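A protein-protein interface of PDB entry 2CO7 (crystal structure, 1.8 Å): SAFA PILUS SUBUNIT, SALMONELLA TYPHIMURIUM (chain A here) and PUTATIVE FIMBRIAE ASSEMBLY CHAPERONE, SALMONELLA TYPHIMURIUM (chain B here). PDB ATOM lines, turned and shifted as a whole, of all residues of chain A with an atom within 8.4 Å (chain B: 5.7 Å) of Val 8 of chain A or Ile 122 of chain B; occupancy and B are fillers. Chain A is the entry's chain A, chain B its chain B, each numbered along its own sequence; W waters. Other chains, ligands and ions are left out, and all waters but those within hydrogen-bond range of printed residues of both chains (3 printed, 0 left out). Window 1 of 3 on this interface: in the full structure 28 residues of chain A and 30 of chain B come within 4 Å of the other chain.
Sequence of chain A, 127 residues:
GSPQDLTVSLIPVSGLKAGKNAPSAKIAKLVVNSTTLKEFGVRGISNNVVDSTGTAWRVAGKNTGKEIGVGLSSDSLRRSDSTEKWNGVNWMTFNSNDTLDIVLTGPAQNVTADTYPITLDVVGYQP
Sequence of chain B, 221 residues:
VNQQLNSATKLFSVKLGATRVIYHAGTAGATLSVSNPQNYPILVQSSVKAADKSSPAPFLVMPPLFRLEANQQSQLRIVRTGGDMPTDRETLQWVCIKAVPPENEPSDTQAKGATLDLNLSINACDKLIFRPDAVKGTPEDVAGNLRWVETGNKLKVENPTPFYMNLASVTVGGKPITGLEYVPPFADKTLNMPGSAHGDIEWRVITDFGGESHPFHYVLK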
ATOM      1  N   ASP A   5      -8.306  29.365  23.724  1.00  0.00           N
ATOM      2  CA  ASP A   5      -9.126  28.310  23.146  1.00  0.00           C
ATOM      3  C   ASP A   5     -10.337  28.858  22.448  1.00  0.00           C
ATOM      4  O   ASP A   5     -10.921  29.840  22.907  1.00  0.00           O
ATOM      5  CB  ASP A   5      -9.508  27.283  24.201  1.00  0.00           C
ATOM      6  CG  ASP A   5      -8.295  26.594  24.783  1.00  0.00           C
ATOM      7  OD1 ASP A   5      -7.399  26.106  24.018  1.00  0.00           O
ATOM      8  OD2 ASP A   5      -8.238  26.579  26.024  1.00  0.00           O
ATOM      9  N   LEU A   6     -10.671  28.244  21.316  1.00  0.00           N
ATOM     10  CA  LEU A   6     -11.866  28.558  20.566  1.00  0.00           C
ATOM     11  C   LEU A   6     -13.109  28.179  21.354  1.00  0.00           C
ATOM     12  O   LEU A   6     -13.287  27.023  21.760  1.00  0.00           O
ATOM     13  CB  LEU A   6     -11.899  27.760  19.254  1.00  0.00           C
ATOM     14  CG  LEU A   6     -11.684  28.437  17.908  1.00  0.00           C
ATOM     15  CD1 LEU A   6     -11.693  27.365  16.827  1.00  0.00           C
ATOM     16  CD2 LEU A   6     -12.751  29.453  17.682  1.00  0.00           C
ATOM     17  N   THR A   7     -13.969  29.169  21.546  1.00  0.00           N
ATOM     18  CA  THR A   7     -15.326  28.954  21.994  1.00  0.00           C
ATOM     19  C   THR A   7     -16.263  29.542  20.942  1.00  0.00           C
ATOM     20  O   THR A   7     -16.128  30.710  20.548  1.00  0.00           O
ATOM     21  CB  THR A   7     -15.607  29.565  23.390  1.00  0.00           C
ATOM     22  OG1 THR A   7     -15.293  30.971  23.402  1.00  0.00           O
ATOM     23  CG2 THR A   7     -14.757  28.872  24.439  1.00  0.00           C
ATOM     24  N   VAL A   8     -17.219  28.728  20.502  1.00  0.00           N
ATOM     25  CA  VAL A   8     -18.101  29.107  19.415  1.00  0.00           C
ATOM     26  C   VAL A   8     -19.527  29.012  19.913  1.00  0.00           C
ATOM     27  O   VAL A   8     -19.871  28.088  20.637  1.00  0.00           O
ATOM     28  CB  VAL A   8     -17.823  28.224  18.181  1.00  0.00           C
ATOM     29  CG1 VAL A   8     -18.778  28.546  17.028  1.00  0.00           C
ATOM     30  CG2 VAL A   8     -16.366  28.427  17.736  1.00  0.00           C
ATOM     31  N   SER A   9     -20.333  30.009  19.556  1.00  0.00           N
ATOM     32  CA  SER A   9     -21.734  30.058  19.939  1.00  0.00           C
ATOM     33  C   SER A   9     -22.573  30.211  18.694  1.00  0.00           C
ATOM     34  O   SER A   9     -22.249  31.004  17.825  1.00  0.00           O
ATOM     35  CB  SER A   9     -21.986  31.248  20.863  1.00  0.00           C
ATOM     36  OG  SER A   9     -21.265  31.125  22.079  1.00  0.00           O
ATOM     37  N   LEU A  10     -23.643  29.434  18.608  1.00  0.00           N
ATOM     38  CA  LEU A  10     -24.628  29.608  17.561  1.00  0.00           C
ATOM     39  C   LEU A  10     -25.954  29.889  18.281  1.00  0.00           C
ATOM     40  O   LEU A  10     -26.459  29.044  19.040  1.00  0.00           O
ATOM     41  CB  LEU A  10     -24.696  28.367  16.664  1.00  0.00           C
ATOM     42  CG  LEU A  10     -25.426  28.436  15.313  1.00  0.00           C
ATOM     43  CD1 LEU A  10     -25.041  29.667  14.490  1.00  0.00           C
ATOM     44  CD2 LEU A  10     -25.203  27.184  14.487  1.00  0.00           C
ATOM     45  N   ILE A  11     -26.454  31.112  18.098  1.00  0.00           N
ATOM     46  CA  ILE A  11     -27.575  31.650  18.869  1.00  0.00           C
ATOM     47  C   ILE A  11     -28.777  31.883  17.944  1.00  0.00           C
ATOM     48  O   ILE A  11     -28.656  32.605  16.950  1.00  0.00           O
ATOM     49  CB  ILE A  11     -27.217  33.010  19.560  1.00  0.00           C
ATOM     50  CG1 ILE A  11     -25.890  32.920  20.342  1.00  0.00           C
ATOM     51  CG2 ILE A  11     -28.360  33.489  20.483  1.00  0.00           C
ATOM     52  CD1 ILE A  11     -25.222  34.272  20.599  1.00  0.00           C
ATOM     53  N   LYS A  29     -27.130  33.510  14.798  1.00  0.00           N
ATOM     54  CA  LYS A  29     -25.996  34.391  15.012  1.00  0.00           C
ATOM     55  C   LYS A  29     -24.837  33.550  15.464  1.00  0.00           C
ATOM     56  O   LYS A  29     -24.974  32.742  16.409  1.00  0.00           O
ATOM     57  CB  LYS A  29     -26.326  35.410  16.098  1.00  0.00           C
ATOM     58  CG  LYS A  29     -25.458  36.655  16.093  1.00  0.00           C
ATOM     59  CD  LYS A  29     -25.508  37.469  17.412  1.00  0.00           C
ATOM     60  CE  LYS A  29     -26.790  37.262  18.205  1.00  0.00           C
ATOM     61  NZ  LYS A  29     -27.167  38.486  19.013  1.00  0.00           N
ATOM     62  N   LEU A  30     -23.708  33.742  14.783  1.00  0.00           N
ATOM     63  CA  LEU A  30     -22.488  33.005  15.069  1.00  0.00           C
ATOM     64  C   LEU A  30     -21.465  33.936  15.714  1.00  0.00           C
ATOM     65  O   LEU A  30     -21.141  35.015  15.183  1.00  0.00           O
ATOM     66  CB  LEU A  30     -21.906  32.393  13.780  1.00  0.00           C
ATOM     67  CG  LEU A  30     -20.575  31.660  13.958  1.00  0.00           C
ATOM     68  CD1 LEU A  30     -20.842  30.325  14.572  1.00  0.00           C
ATOM     69  CD2 LEU A  30     -19.843  31.496  12.633  1.00  0.00           C
ATOM     70  N   VAL A  31     -20.965  33.517  16.870  1.00  0.00           N
ATOM     71  CA  VAL A  31     -19.873  34.218  17.543  1.00  0.00           C
ATOM     72  C   VAL A  31     -18.719  33.255  17.794  1.00  0.00           C
ATOM     73  O   VAL A  31     -18.914  32.157  18.316  1.00  0.00           O
ATOM     74  CB  VAL A  31     -20.319  34.789  18.919  1.00  0.00           C
ATOM     75  CG1 VAL A  31     -19.200  35.614  19.515  1.00  0.00           C
ATOM     76  CG2 VAL A  31     -21.589  35.624  18.788  1.00  0.00           C
ATOM     77  N   VAL A  32     -17.514  33.671  17.424  1.00  0.00           N
ATOM     78  CA  VAL A  32     -16.342  32.868  17.661  1.00  0.00           C
ATOM     79  C   VAL A  32     -15.432  33.690  18.574  1.00  0.00           C
ATOM     80  O   VAL A  32     -15.080  34.841  18.263  1.00  0.00           O
ATOM     81  CB  VAL A  32     -15.647  32.496  16.314  1.00  0.00           C
ATOM     82  CG1 VAL A  32     -14.378  31.725  16.554  1.00  0.00           C
ATOM     83  CG2 VAL A  32     -16.596  31.713  15.415  1.00  0.00           C
ATOM     84  N   ASN A  33     -15.078  33.121  19.722  1.00  0.00           N
ATOM     85  CA  ASN A  33     -14.255  33.831  20.685  1.00  0.00           C
ATOM     86  C   ASN A  33     -12.919  33.153  20.944  1.00  0.00           C
ATOM     87  O   ASN A  33     -12.850  31.943  21.064  1.00  0.00           O
ATOM     88  CB  ASN A  33     -15.004  34.030  21.988  1.00  0.00           C
ATOM     89  CG  ASN A  33     -16.187  34.962  21.834  1.00  0.00           C
ATOM     90  OD1 ASN A  33     -17.314  34.574  22.108  1.00  0.00           O
ATOM     91  ND2 ASN A  33     -15.938  36.191  21.364  1.00  0.00           N
ATOM     92  N   SER A  34     -11.869  33.967  20.982  1.00  0.00           N
ATOM     93  CA  SER A  34     -10.553  33.530  21.419  1.00  0.00           C
ATOM     94  C   SER A  34      -9.766  34.816  21.615  1.00  0.00           C
ATOM     95  O   SER A  34      -9.916  35.757  20.814  1.00  0.00           O
ATOM     96  CB  SER A  34      -9.892  32.672  20.324  1.00  0.00           C
ATOM     97  OG  SER A  34      -8.493  32.548  20.528  1.00  0.00           O
ATOM     98  N   LEU A  37      -6.656  34.019  18.701  1.00  0.00           N
ATOM     99  CA  LEU A  37      -6.915  33.902  17.263  1.00  0.00           C
ATOM    100  C   LEU A  37      -6.996  35.266  16.651  1.00  0.00           C
ATOM    101  O   LEU A  37      -7.521  36.201  17.256  1.00  0.00           O
ATOM    102  CB  LEU A  37      -8.238  33.193  16.953  1.00  0.00           C
ATOM    103  CG  LEU A  37      -8.342  31.685  16.940  1.00  0.00           C
ATOM    104  CD1 LEU A  37      -9.759  31.373  16.415  1.00  0.00           C
ATOM    105  CD2 LEU A  37      -7.269  31.031  16.034  1.00  0.00           C
ATOM    106  N   PHE A  40     -10.874  33.343  11.848  1.00  0.00           N
ATOM    107  CA  PHE A  40     -11.406  31.970  11.729  1.00  0.00           C
ATOM    108  C   PHE A  40     -12.058  31.737  10.377  1.00  0.00           C
ATOM    109  O   PHE A  40     -12.407  32.712   9.686  1.00  0.00           O
ATOM    110  CB  PHE A  40     -12.430  31.717  12.852  1.00  0.00           C
ATOM    111  CG  PHE A  40     -13.671  32.583  12.749  1.00  0.00           C
ATOM    112  CD1 PHE A  40     -14.810  32.102  12.085  1.00  0.00           C
ATOM    113  CD2 PHE A  40     -13.727  33.833  13.369  1.00  0.00           C
ATOM    114  CE1 PHE A  40     -15.972  32.874  11.991  1.00  0.00           C
ATOM    115  CE2 PHE A  40     -14.901  34.609  13.299  1.00  0.00           C
ATOM    116  CZ  PHE A  40     -16.013  34.140  12.606  1.00  0.00           C
ATOM    117  N   GLY A  41     -12.237  30.464  10.018  1.00  0.00           N
ATOM    118  CA  GLY A  41     -12.961  30.082   8.824  1.00  0.00           C
ATOM    119  C   GLY A  41     -14.258  29.469   9.299  1.00  0.00           C
ATOM    120  O   GLY A  41     -14.295  28.889  10.383  1.00  0.00           O
ATOM    121  N   VAL A  42     -15.323  29.639   8.514  1.00  0.00           N
ATOM    122  CA  VAL A  42     -16.605  28.968   8.794  1.00  0.00           C
ATOM    123  C   VAL A  42     -17.289  28.501   7.514  1.00  0.00           C
ATOM    124  O   VAL A  42     -17.262  29.216   6.504  1.00  0.00           O
ATOM    125  CB  VAL A  42     -17.549  29.813   9.644  1.00  0.00           C
ATOM    126  CG1 VAL A  42     -17.974  31.089   8.899  1.00  0.00           C
ATOM    127  CG2 VAL A  42     -18.769  28.989  10.078  1.00  0.00           C
ATOM    128  N   ILE A  45     -22.519  23.053   6.862  1.00  0.00           N
ATOM    129  CA  ILE A  45     -22.420  21.628   6.557  1.00  0.00           C
ATOM    130  C   ILE A  45     -23.786  21.153   6.148  1.00  0.00           C
ATOM    131  O   ILE A  45     -24.762  21.321   6.883  1.00  0.00           O
ATOM    132  CB  ILE A  45     -21.921  20.777   7.758  1.00  0.00           C
ATOM    133  CG1 ILE A  45     -20.461  21.100   8.081  1.00  0.00           C
ATOM    134  CG2 ILE A  45     -22.095  19.278   7.455  1.00  0.00           C
ATOM    135  CD1 ILE A  45     -19.966  20.521   9.403  1.00  0.00           C
ATOM    136  N   TRP A  91     -12.578  28.203   2.159  1.00  0.00           N
ATOM    137  CA  TRP A  91     -13.150  28.770   3.386  1.00  0.00           C
ATOM    138  C   TRP A  91     -13.069  30.275   3.318  1.00  0.00           C
ATOM    139  O   TRP A  91     -12.027  30.828   2.966  1.00  0.00           O
ATOM    140  CB  TRP A  91     -12.302  28.374   4.594  1.00  0.00           C
ATOM    141  CG  TRP A  91     -12.293  26.948   4.963  1.00  0.00           C
ATOM    142  CD1 TRP A  91     -11.548  25.950   4.386  1.00  0.00           C
ATOM    143  CD2 TRP A  91     -12.995  26.340   6.066  1.00  0.00           C
ATOM    144  NE1 TRP A  91     -11.768  24.762   5.037  1.00  0.00           N
ATOM    145  CE2 TRP A  91     -12.647  24.973   6.073  1.00  0.00           C
ATOM    146  CE3 TRP A  91     -13.902  26.822   7.038  1.00  0.00           C
ATOM    147  CZ2 TRP A  91     -13.175  24.057   7.016  1.00  0.00           C
ATOM    148  CZ3 TRP A  91     -14.438  25.904   7.968  1.00  0.00           C
ATOM    149  CH2 TRP A  91     -14.062  24.546   7.945  1.00  0.00           C
ATOM    150  N   LEU A 120     -22.772  24.308  11.417  1.00  0.00           N
ATOM    151  CA  LEU A 120     -21.586  25.072  10.996  1.00  0.00           C
ATOM    152  C   LEU A 120     -20.300  24.436  11.493  1.00  0.00           C
ATOM    153  O   LEU A 120     -20.246  23.952  12.616  1.00  0.00           O
ATOM    154  CB  LEU A 120     -21.680  26.527  11.483  1.00  0.00           C
ATOM    155  CG  LEU A 120     -22.957  27.315  11.102  1.00  0.00           C
ATOM    156  CD1 LEU A 120     -22.931  28.703  11.732  1.00  0.00           C
ATOM    157  CD2 LEU A 120     -23.109  27.433   9.608  1.00  0.00           C
ATOM    158  N   ASP A 121     -19.283  24.430  10.634  1.00  0.00           N
ATOM    159  CA  ASP A 121     -17.951  23.941  10.955  1.00  0.00           C
ATOM    160  C   ASP A 121     -16.997  25.140  11.011  1.00  0.00           C
ATOM    161  O   ASP A 121     -16.953  25.925  10.084  1.00  0.00           O
ATOM    162  CB  ASP A 121     -17.486  22.982   9.868  1.00  0.00           C
ATOM    163  CG  ASP A 121     -16.246  22.209  10.258  1.00  0.00           C
ATOM    164  OD1 ASP A 121     -15.580  21.670   9.334  1.00  0.00           O
ATOM    165  OD2 ASP A 121     -15.948  22.101  11.481  1.00  0.00           O
ATOM    166  N   VAL A 122     -16.255  25.284  12.105  1.00  0.00           N
ATOM    167  CA  VAL A 122     -15.386  26.453  12.319  1.00  0.00           C
ATOM    168  C   VAL A 122     -13.943  25.950  12.459  1.00  0.00           C
ATOM    169  O   VAL A 122     -13.719  24.916  13.080  1.00  0.00           O
ATOM    170  CB  VAL A 122     -15.793  27.231  13.612  1.00  0.00           C
ATOM    171  CG1 VAL A 122     -14.764  28.337  13.982  1.00  0.00           C
ATOM    172  CG2 VAL A 122     -17.180  27.844  13.458  1.00  0.00           C
ATOM    173  N   VAL A 123     -12.985  26.689  11.877  1.00  0.00           N
ATOM    174  CA  VAL A 123     -11.580  26.358  12.039  1.00  0.00           C
ATOM    175  C   VAL A 123     -10.824  27.618  12.471  1.00  0.00           C
ATOM    176  O   VAL A 123     -11.105  28.723  11.985  1.00  0.00           O
ATOM    177  CB  VAL A 123     -10.973  25.737  10.755  1.00  0.00           C
ATOM    178  CG1 VAL A 123     -11.129  26.659   9.546  1.00  0.00           C
ATOM    179  CG2 VAL A 123      -9.439  25.301  10.990  1.00  0.00           C
ATOM    180  N   GLY A 124      -9.869  27.445  13.380  1.00  0.00           N
ATOM    181  CA  GLY A 124      -8.949  28.536  13.753  1.00  0.00           C
ATOM    182  C   GLY A 124      -7.516  28.020  13.776  1.00  0.00           C
ATOM    183  O   GLY A 124      -7.230  27.017  14.422  1.00  0.00           O
ATOM    184  N   LYS B  10     -26.445  27.050  21.058  1.00  0.00           N
ATOM    185  CA  LYS B  10     -25.445  25.992  21.042  1.00  0.00           C
ATOM    186  C   LYS B  10     -24.074  26.587  21.304  1.00  0.00           C
ATOM    187  O   LYS B  10     -23.621  27.481  20.577  1.00  0.00           O
ATOM    188  CB  LYS B  10     -25.412  25.257  19.696  1.00  0.00           C
ATOM    189  CG  LYS B  10     -24.336  24.148  19.608  1.00  0.00           C
ATOM    190  CD  LYS B  10     -24.579  23.023  20.628  1.00  0.00           C
ATOM    191  CE  LYS B  10     -23.377  22.066  20.796  1.00  0.00           C
ATOM    192  NZ  LYS B  10     -23.869  20.677  21.195  1.00  0.00           N
ATOM    193  N   LEU B  11     -23.433  26.087  22.353  1.00  0.00           N
ATOM    194  CA  LEU B  11     -22.091  26.486  22.712  1.00  0.00           C
ATOM    195  C   LEU B  11     -21.185  25.300  22.487  1.00  0.00           C
ATOM    196  O   LEU B  11     -21.571  24.150  22.750  1.00  0.00           O
ATOM    197  CB  LEU B  11     -21.984  26.884  24.186  1.00  0.00           C
ATOM    198  CG  LEU B  11     -22.918  27.955  24.749  1.00  0.00           C
ATOM    199  CD1 LEU B  11     -22.512  28.239  26.174  1.00  0.00           C
ATOM    200  CD2 LEU B  11     -22.819  29.221  23.891  1.00  0.00           C
ATOM    201  N   PHE B  12     -19.982  25.578  22.021  1.00  0.00           N
ATOM    202  CA  PHE B  12     -19.023  24.492  21.796  1.00  0.00           C
ATOM    203  C   PHE B  12     -17.600  24.976  21.843  1.00  0.00           C
ATOM    204  O   PHE B  12     -17.285  26.046  21.306  1.00  0.00           O
ATOM    205  CB  PHE B  12     -19.330  23.745  20.488  1.00  0.00           C
ATOM    206  CG  PHE B  12     -18.737  22.364  20.437  1.00  0.00           C
ATOM    207  CD1 PHE B  12     -19.135  21.403  21.360  1.00  0.00           C
ATOM    208  CD2 PHE B  12     -17.791  22.032  19.469  1.00  0.00           C
ATOM    209  CE1 PHE B  12     -18.600  20.128  21.339  1.00  0.00           C
ATOM    210  CE2 PHE B  12     -17.231  20.741  19.447  1.00  0.00           C
ATOM    211  CZ  PHE B  12     -17.655  19.803  20.393  1.00  0.00           C
ATOM    212  N   SER B  13     -16.736  24.191  22.508  1.00  0.00           N
ATOM    213  CA  SER B  13     -15.341  24.557  22.697  1.00  0.00           C
ATOM    214  C   SER B  13     -14.455  23.296  22.788  1.00  0.00           C
ATOM    215  O   SER B  13     -14.941  22.217  23.085  1.00  0.00           O
ATOM    216  CB  SER B  13     -15.163  25.385  23.987  1.00  0.00           C
ATOM    217  OG  SER B  13     -13.792  25.760  24.125  1.00  0.00           O
ATOM    218  N   VAL B  14     -13.168  23.441  22.499  1.00  0.00           N
ATOM    219  CA  VAL B  14     -12.170  22.395  22.784  1.00  0.00           C
ATOM    220  C   VAL B  14     -10.971  23.100  23.412  1.00  0.00           C
ATOM    221  O   VAL B  14     -10.679  24.251  23.057  1.00  0.00           O
ATOM    222  CB  VAL B  14     -11.789  21.543  21.518  1.00  0.00           C
ATOM    223  CG1 VAL B  14     -10.985  22.369  20.473  1.00  0.00           C
ATOM    224  CG2 VAL B  14     -11.010  20.306  21.912  1.00  0.00           C
ATOM    225  N   ILE B  97      -6.909  19.668  15.823  1.00  0.00           N
ATOM    226  CA  ILE B  97      -7.776  18.868  16.673  1.00  0.00           C
ATOM    227  C   ILE B  97      -9.177  19.192  16.216  1.00  0.00           C
ATOM    228  O   ILE B  97      -9.588  20.353  16.340  1.00  0.00           O
ATOM    229  CB  ILE B  97      -7.635  19.335  18.164  1.00  0.00           C
ATOM    230  CG1 ILE B  97      -6.210  19.151  18.699  1.00  0.00           C
ATOM    231  CG2 ILE B  97      -8.689  18.680  19.083  1.00  0.00           C
ATOM    232  CD1 ILE B  97      -5.603  17.843  18.410  1.00  0.00           C
ATOM    233  N   LYS B  98      -9.865  18.200  15.649  1.00  0.00           N
ATOM    234  CA  LYS B  98     -11.269  18.337  15.240  1.00  0.00           C
ATOM    235  C   LYS B  98     -12.151  17.743  16.325  1.00  0.00           C
ATOM    236  O   LYS B  98     -11.967  16.571  16.712  1.00  0.00           O
ATOM    237  CB  LYS B  98     -11.555  17.576  13.939  1.00  0.00           C
ATOM    238  CG  LYS B  98     -13.017  17.741  13.452  1.00  0.00           C
ATOM    239  CD  LYS B  98     -13.355  16.871  12.230  1.00  0.00           C
ATOM    240  CE  LYS B  98     -12.427  17.175  11.052  1.00  0.00           C
ATOM    241  NZ  LYS B  98     -12.746  18.529  10.486  1.00  0.00           N
ATOM    242  N   ALA B  99     -13.119  18.537  16.781  1.00  0.00           N
ATOM    243  CA  ALA B  99     -14.003  18.109  17.879  1.00  0.00           C
ATOM    244  C   ALA B  99     -15.431  18.160  17.363  1.00  0.00           C
ATOM    245  O   ALA B  99     -15.857  19.137  16.743  1.00  0.00           O
ATOM    246  CB  ALA B  99     -13.822  18.988  19.114  1.00  0.00           C
ATOM    247  N   VAL B 100     -16.156  17.087  17.641  1.00  0.00           N
ATOM    248  CA  VAL B 100     -17.482  16.855  17.085  1.00  0.00           C
ATOM    249  C   VAL B 100     -18.435  16.422  18.217  1.00  0.00           C
ATOM    250  O   VAL B 100     -18.205  15.392  18.856  1.00  0.00           O
ATOM    251  CB  VAL B 100     -17.401  15.784  15.959  1.00  0.00           C
ATOM    252  CG1 VAL B 100     -18.749  15.420  15.462  1.00  0.00           C
ATOM    253  CG2 VAL B 100     -16.501  16.300  14.801  1.00  0.00           C
ATOM    254  N   LEU B 120     -22.602  22.359  16.056  1.00  0.00           N
ATOM    255  CA  LEU B 120     -21.323  22.897  15.654  1.00  0.00           C
ATOM    256  C   LEU B 120     -20.286  21.797  15.603  1.00  0.00           C
ATOM    257  O   LEU B 120     -20.406  20.797  16.294  1.00  0.00           O
ATOM    258  CB  LEU B 120     -20.899  23.950  16.668  1.00  0.00           C
ATOM    259  CG  LEU B 120     -21.659  25.286  16.743  1.00  0.00           C
ATOM    260  CD1 LEU B 120     -21.246  26.047  18.004  1.00  0.00           C
ATOM    261  CD2 LEU B 120     -21.426  26.164  15.497  1.00  0.00           C
ATOM    262  N   SER B 121     -19.261  21.981  14.788  1.00  0.00           N
ATOM    263  CA  SER B 121     -18.048  21.219  14.975  1.00  0.00           C
ATOM    264  C   SER B 121     -16.898  22.210  14.852  1.00  0.00           C
ATOM    265  O   SER B 121     -17.022  23.228  14.181  1.00  0.00           O
ATOM    266  CB  SER B 121     -17.932  20.103  13.945  1.00  0.00           C
ATOM    267  OG  SER B 121     -17.679  20.632  12.671  1.00  0.00           O
ATOM    268  N   ILE B 122     -15.791  21.937  15.526  1.00  0.00           N
ATOM    269  CA  ILE B 122     -14.705  22.915  15.539  1.00  0.00           C
ATOM    270  C   ILE B 122     -13.355  22.265  15.297  1.00  0.00           C
ATOM    271  O   ILE B 122     -13.183  21.072  15.549  1.00  0.00           O
ATOM    272  CB  ILE B 122     -14.739  23.852  16.803  1.00  0.00           C
ATOM    273  CG1 ILE B 122     -14.536  23.065  18.086  1.00  0.00           C
ATOM    274  CG2 ILE B 122     -16.133  24.579  16.944  1.00  0.00           C
ATOM    275  CD1 ILE B 122     -14.557  23.978  19.402  1.00  0.00           C
ATOM    276  N   ASN B 123     -12.424  23.060  14.773  1.00  0.00           N
ATOM    277  CA  ASN B 123     -11.087  22.578  14.431  1.00  0.00           C
ATOM    278  C   ASN B 123     -10.107  23.587  14.953  1.00  0.00           C
ATOM    279  O   ASN B 123     -10.130  24.753  14.530  1.00  0.00           O
ATOM    280  CB  ASN B 123     -10.921  22.449  12.914  1.00  0.00           C
ATOM    281  CG  ASN B 123     -11.966  21.601  12.291  1.00  0.00           C
ATOM    282  OD1 ASN B 123     -11.788  20.388  12.192  1.00  0.00           O
ATOM    283  ND2 ASN B 123     -13.092  22.212  11.886  1.00  0.00           N
ATOM    284  N   ALA B 124      -9.306  23.182  15.941  1.00  0.00           N
ATOM    285  CA  ALA B 124      -8.328  24.070  16.526  1.00  0.00           C
ATOM    286  C   ALA B 124      -6.961  23.594  16.090  1.00  0.00           C
ATOM    287  O   ALA B 124      -6.589  22.465  16.397  1.00  0.00           O
ATOM    288  CB  ALA B 124      -8.438  24.046  18.098  1.00  0.00           C
HETATM  289  O   HOH W   1      -8.961  25.807  21.447  1.00  0.00           O
HETATM  290  O   HOH W   2     -12.885  20.794   8.923  1.00  0.00           O
HETATM  291  O   HOH W   3     -15.468  18.540  10.162  1.00  0.00           O
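The backbone carbonyl oxygen (O) of Val 31 of chain A lies within hydrogen-bond range of the backbone NH (N) of Ser 9 of chain A (2.9 Å).
O of Val 123 of chain A is in hydrogen-bond range of N of Gly 41 of chain A, 2.9 Å away.
The backbone carbonyl oxygen of Thr 7 of chain A lies within hydrogen-bond range of the backbone NH of Asn 33 of chain A (2.8 Å).
Hydrophobic or aromatic side chains of chain A that line the printed part of chain B: Leu 6, Val 8, Ile 45 and Val 123.
Printed residues of chain B that touch a printed residue of chain A: Lys 10, Leu 11, Phe 12, Ser 13, Val 14, Leu 120, Ser 121, Ile 122, Asn 123 and Ala 124.
Among the printed residues, no Asp or Glu carboxylate lies within 4 Å of a Lys or Arg side-chain nitrogen of the other chain.
The backbone carbonyl oxygen of Leu 6 of chain A lies within hydrogen-bond range of the side-chain hydroxyl of Ser 13 of chain B (2.7 Å).
The backbone NH (N) of Val 8 of chain A lies within hydrogen-bond range of the backbone carbonyl oxygen (O) of Phe 12 of chain B (2.8 Å).
The side-chain hydroxyl of Ser 121 of chain B sits at hydrogen-bond distance from the side-chain carboxylate of Asp 121 of chain A, 2.6 Å away.
N of Val 122 of chain A lies within hydrogen-bond range of O of Ser 121 of chain B (3.0 Å).
The backbone NH (N) of Leu 10 of chain A sits at hydrogen-bond distance from the backbone carbonyl oxygen (O) of Lys 10 of chain B.
The backbone NH (N) of Gly 124 of chain A is in hydrogen-bond range of the backbone carbonyl oxygen (O) of Asn 123 of chain B, at 2.9 Å.
The side-chain amide nitrogen (ND2) of Asn 123 of chain B sits at hydrogen-bond distance from the side-chain carboxylate (OD2) of Asp 121 of chain A (2.9 Å).
O of Val 122 of chain A lies within hydrogen-bond range of N of Asn 123 of chain B (2.8 Å).
The backbone carbonyl oxygen of Leu 120 of chain A lies within hydrogen-bond range of the backbone NH of Ser 121 of chain B, 3.1 Å away.
Water W3 bridges NZ of Lys 98 of chain B (2.7 Å) and OD1 of Asp 121 of chain A (3.2 Å).
Water W2 lies within hydrogen-bond range of NZ of Lys 98 of chain B (2.8 Å), OD1 of Asp 121 of chain A (2.9 Å) and ND2 of Asn 123 of chain B (3.3 Å).
Water W1 lies within hydrogen-bond range of O of Val 14 of chain B (2.8 Å), N of Leu 6 of chain A (3.0 Å) and OD1 of Asp 5 of chain A (3.0 Å).
O of Val 14 of chain B touches CB of Asp 5 of chain A, at 3.4 Å.
Asn 123 of chain B touches Leu 6 of chain A.
Val 8 of chain A touches Leu 120 of chain B.
Ile 122 of chain B touches Val 8 of chain A.
CA of Ser 9 of chain A touches O of Lys 10 of chain B, at 3.3 Å.
Leu 11 of chain B touches Ser 9 of chain A (CD2 to OG, 3.1 Å).
Ser 121 of chain B touches Ile 45 of chain A (OG to CD1, 3.99 Å).
Of the printed residues of chain B, Leu 6 of chain A touches Ser 13 (2.7 Å), Val 14 (3.7 Å) and Asn 123 (3.8 Å).
Val 8 of chain A touches just these residues of chain B: Lys 10 (3.8 Å), Leu 11 (3.4 Å), Phe 12 (2.8 Å), Leu 120 (3.6 Å) and Ile 122 (3.9 Å).
Phe 40 of chain A touches none of the printed residues of chain B.
Of the printed residues of chain A, Phe 12 of chain B touches Thr 7 and Val 8.
Of the printed residues of chain A, Ser 13 of chain B touches Leu 6 (2.7 Å) and Thr 7 (3.3 Å).
Ile 122 of chain B touches just these residues of chain A: Val 8 (3.9 Å) and Val 122 (3.3 Å).
Asn 123 of chain B touches five residues of chain A.
The nearest residue of chain B that does not touch Val 8 of chain A is Ser 13 of chain B (5.0 Å).
The nearest printed residue of chain A that does not touch Ile 122 of chain B is Asp 121 of chain A (4.1 Å).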
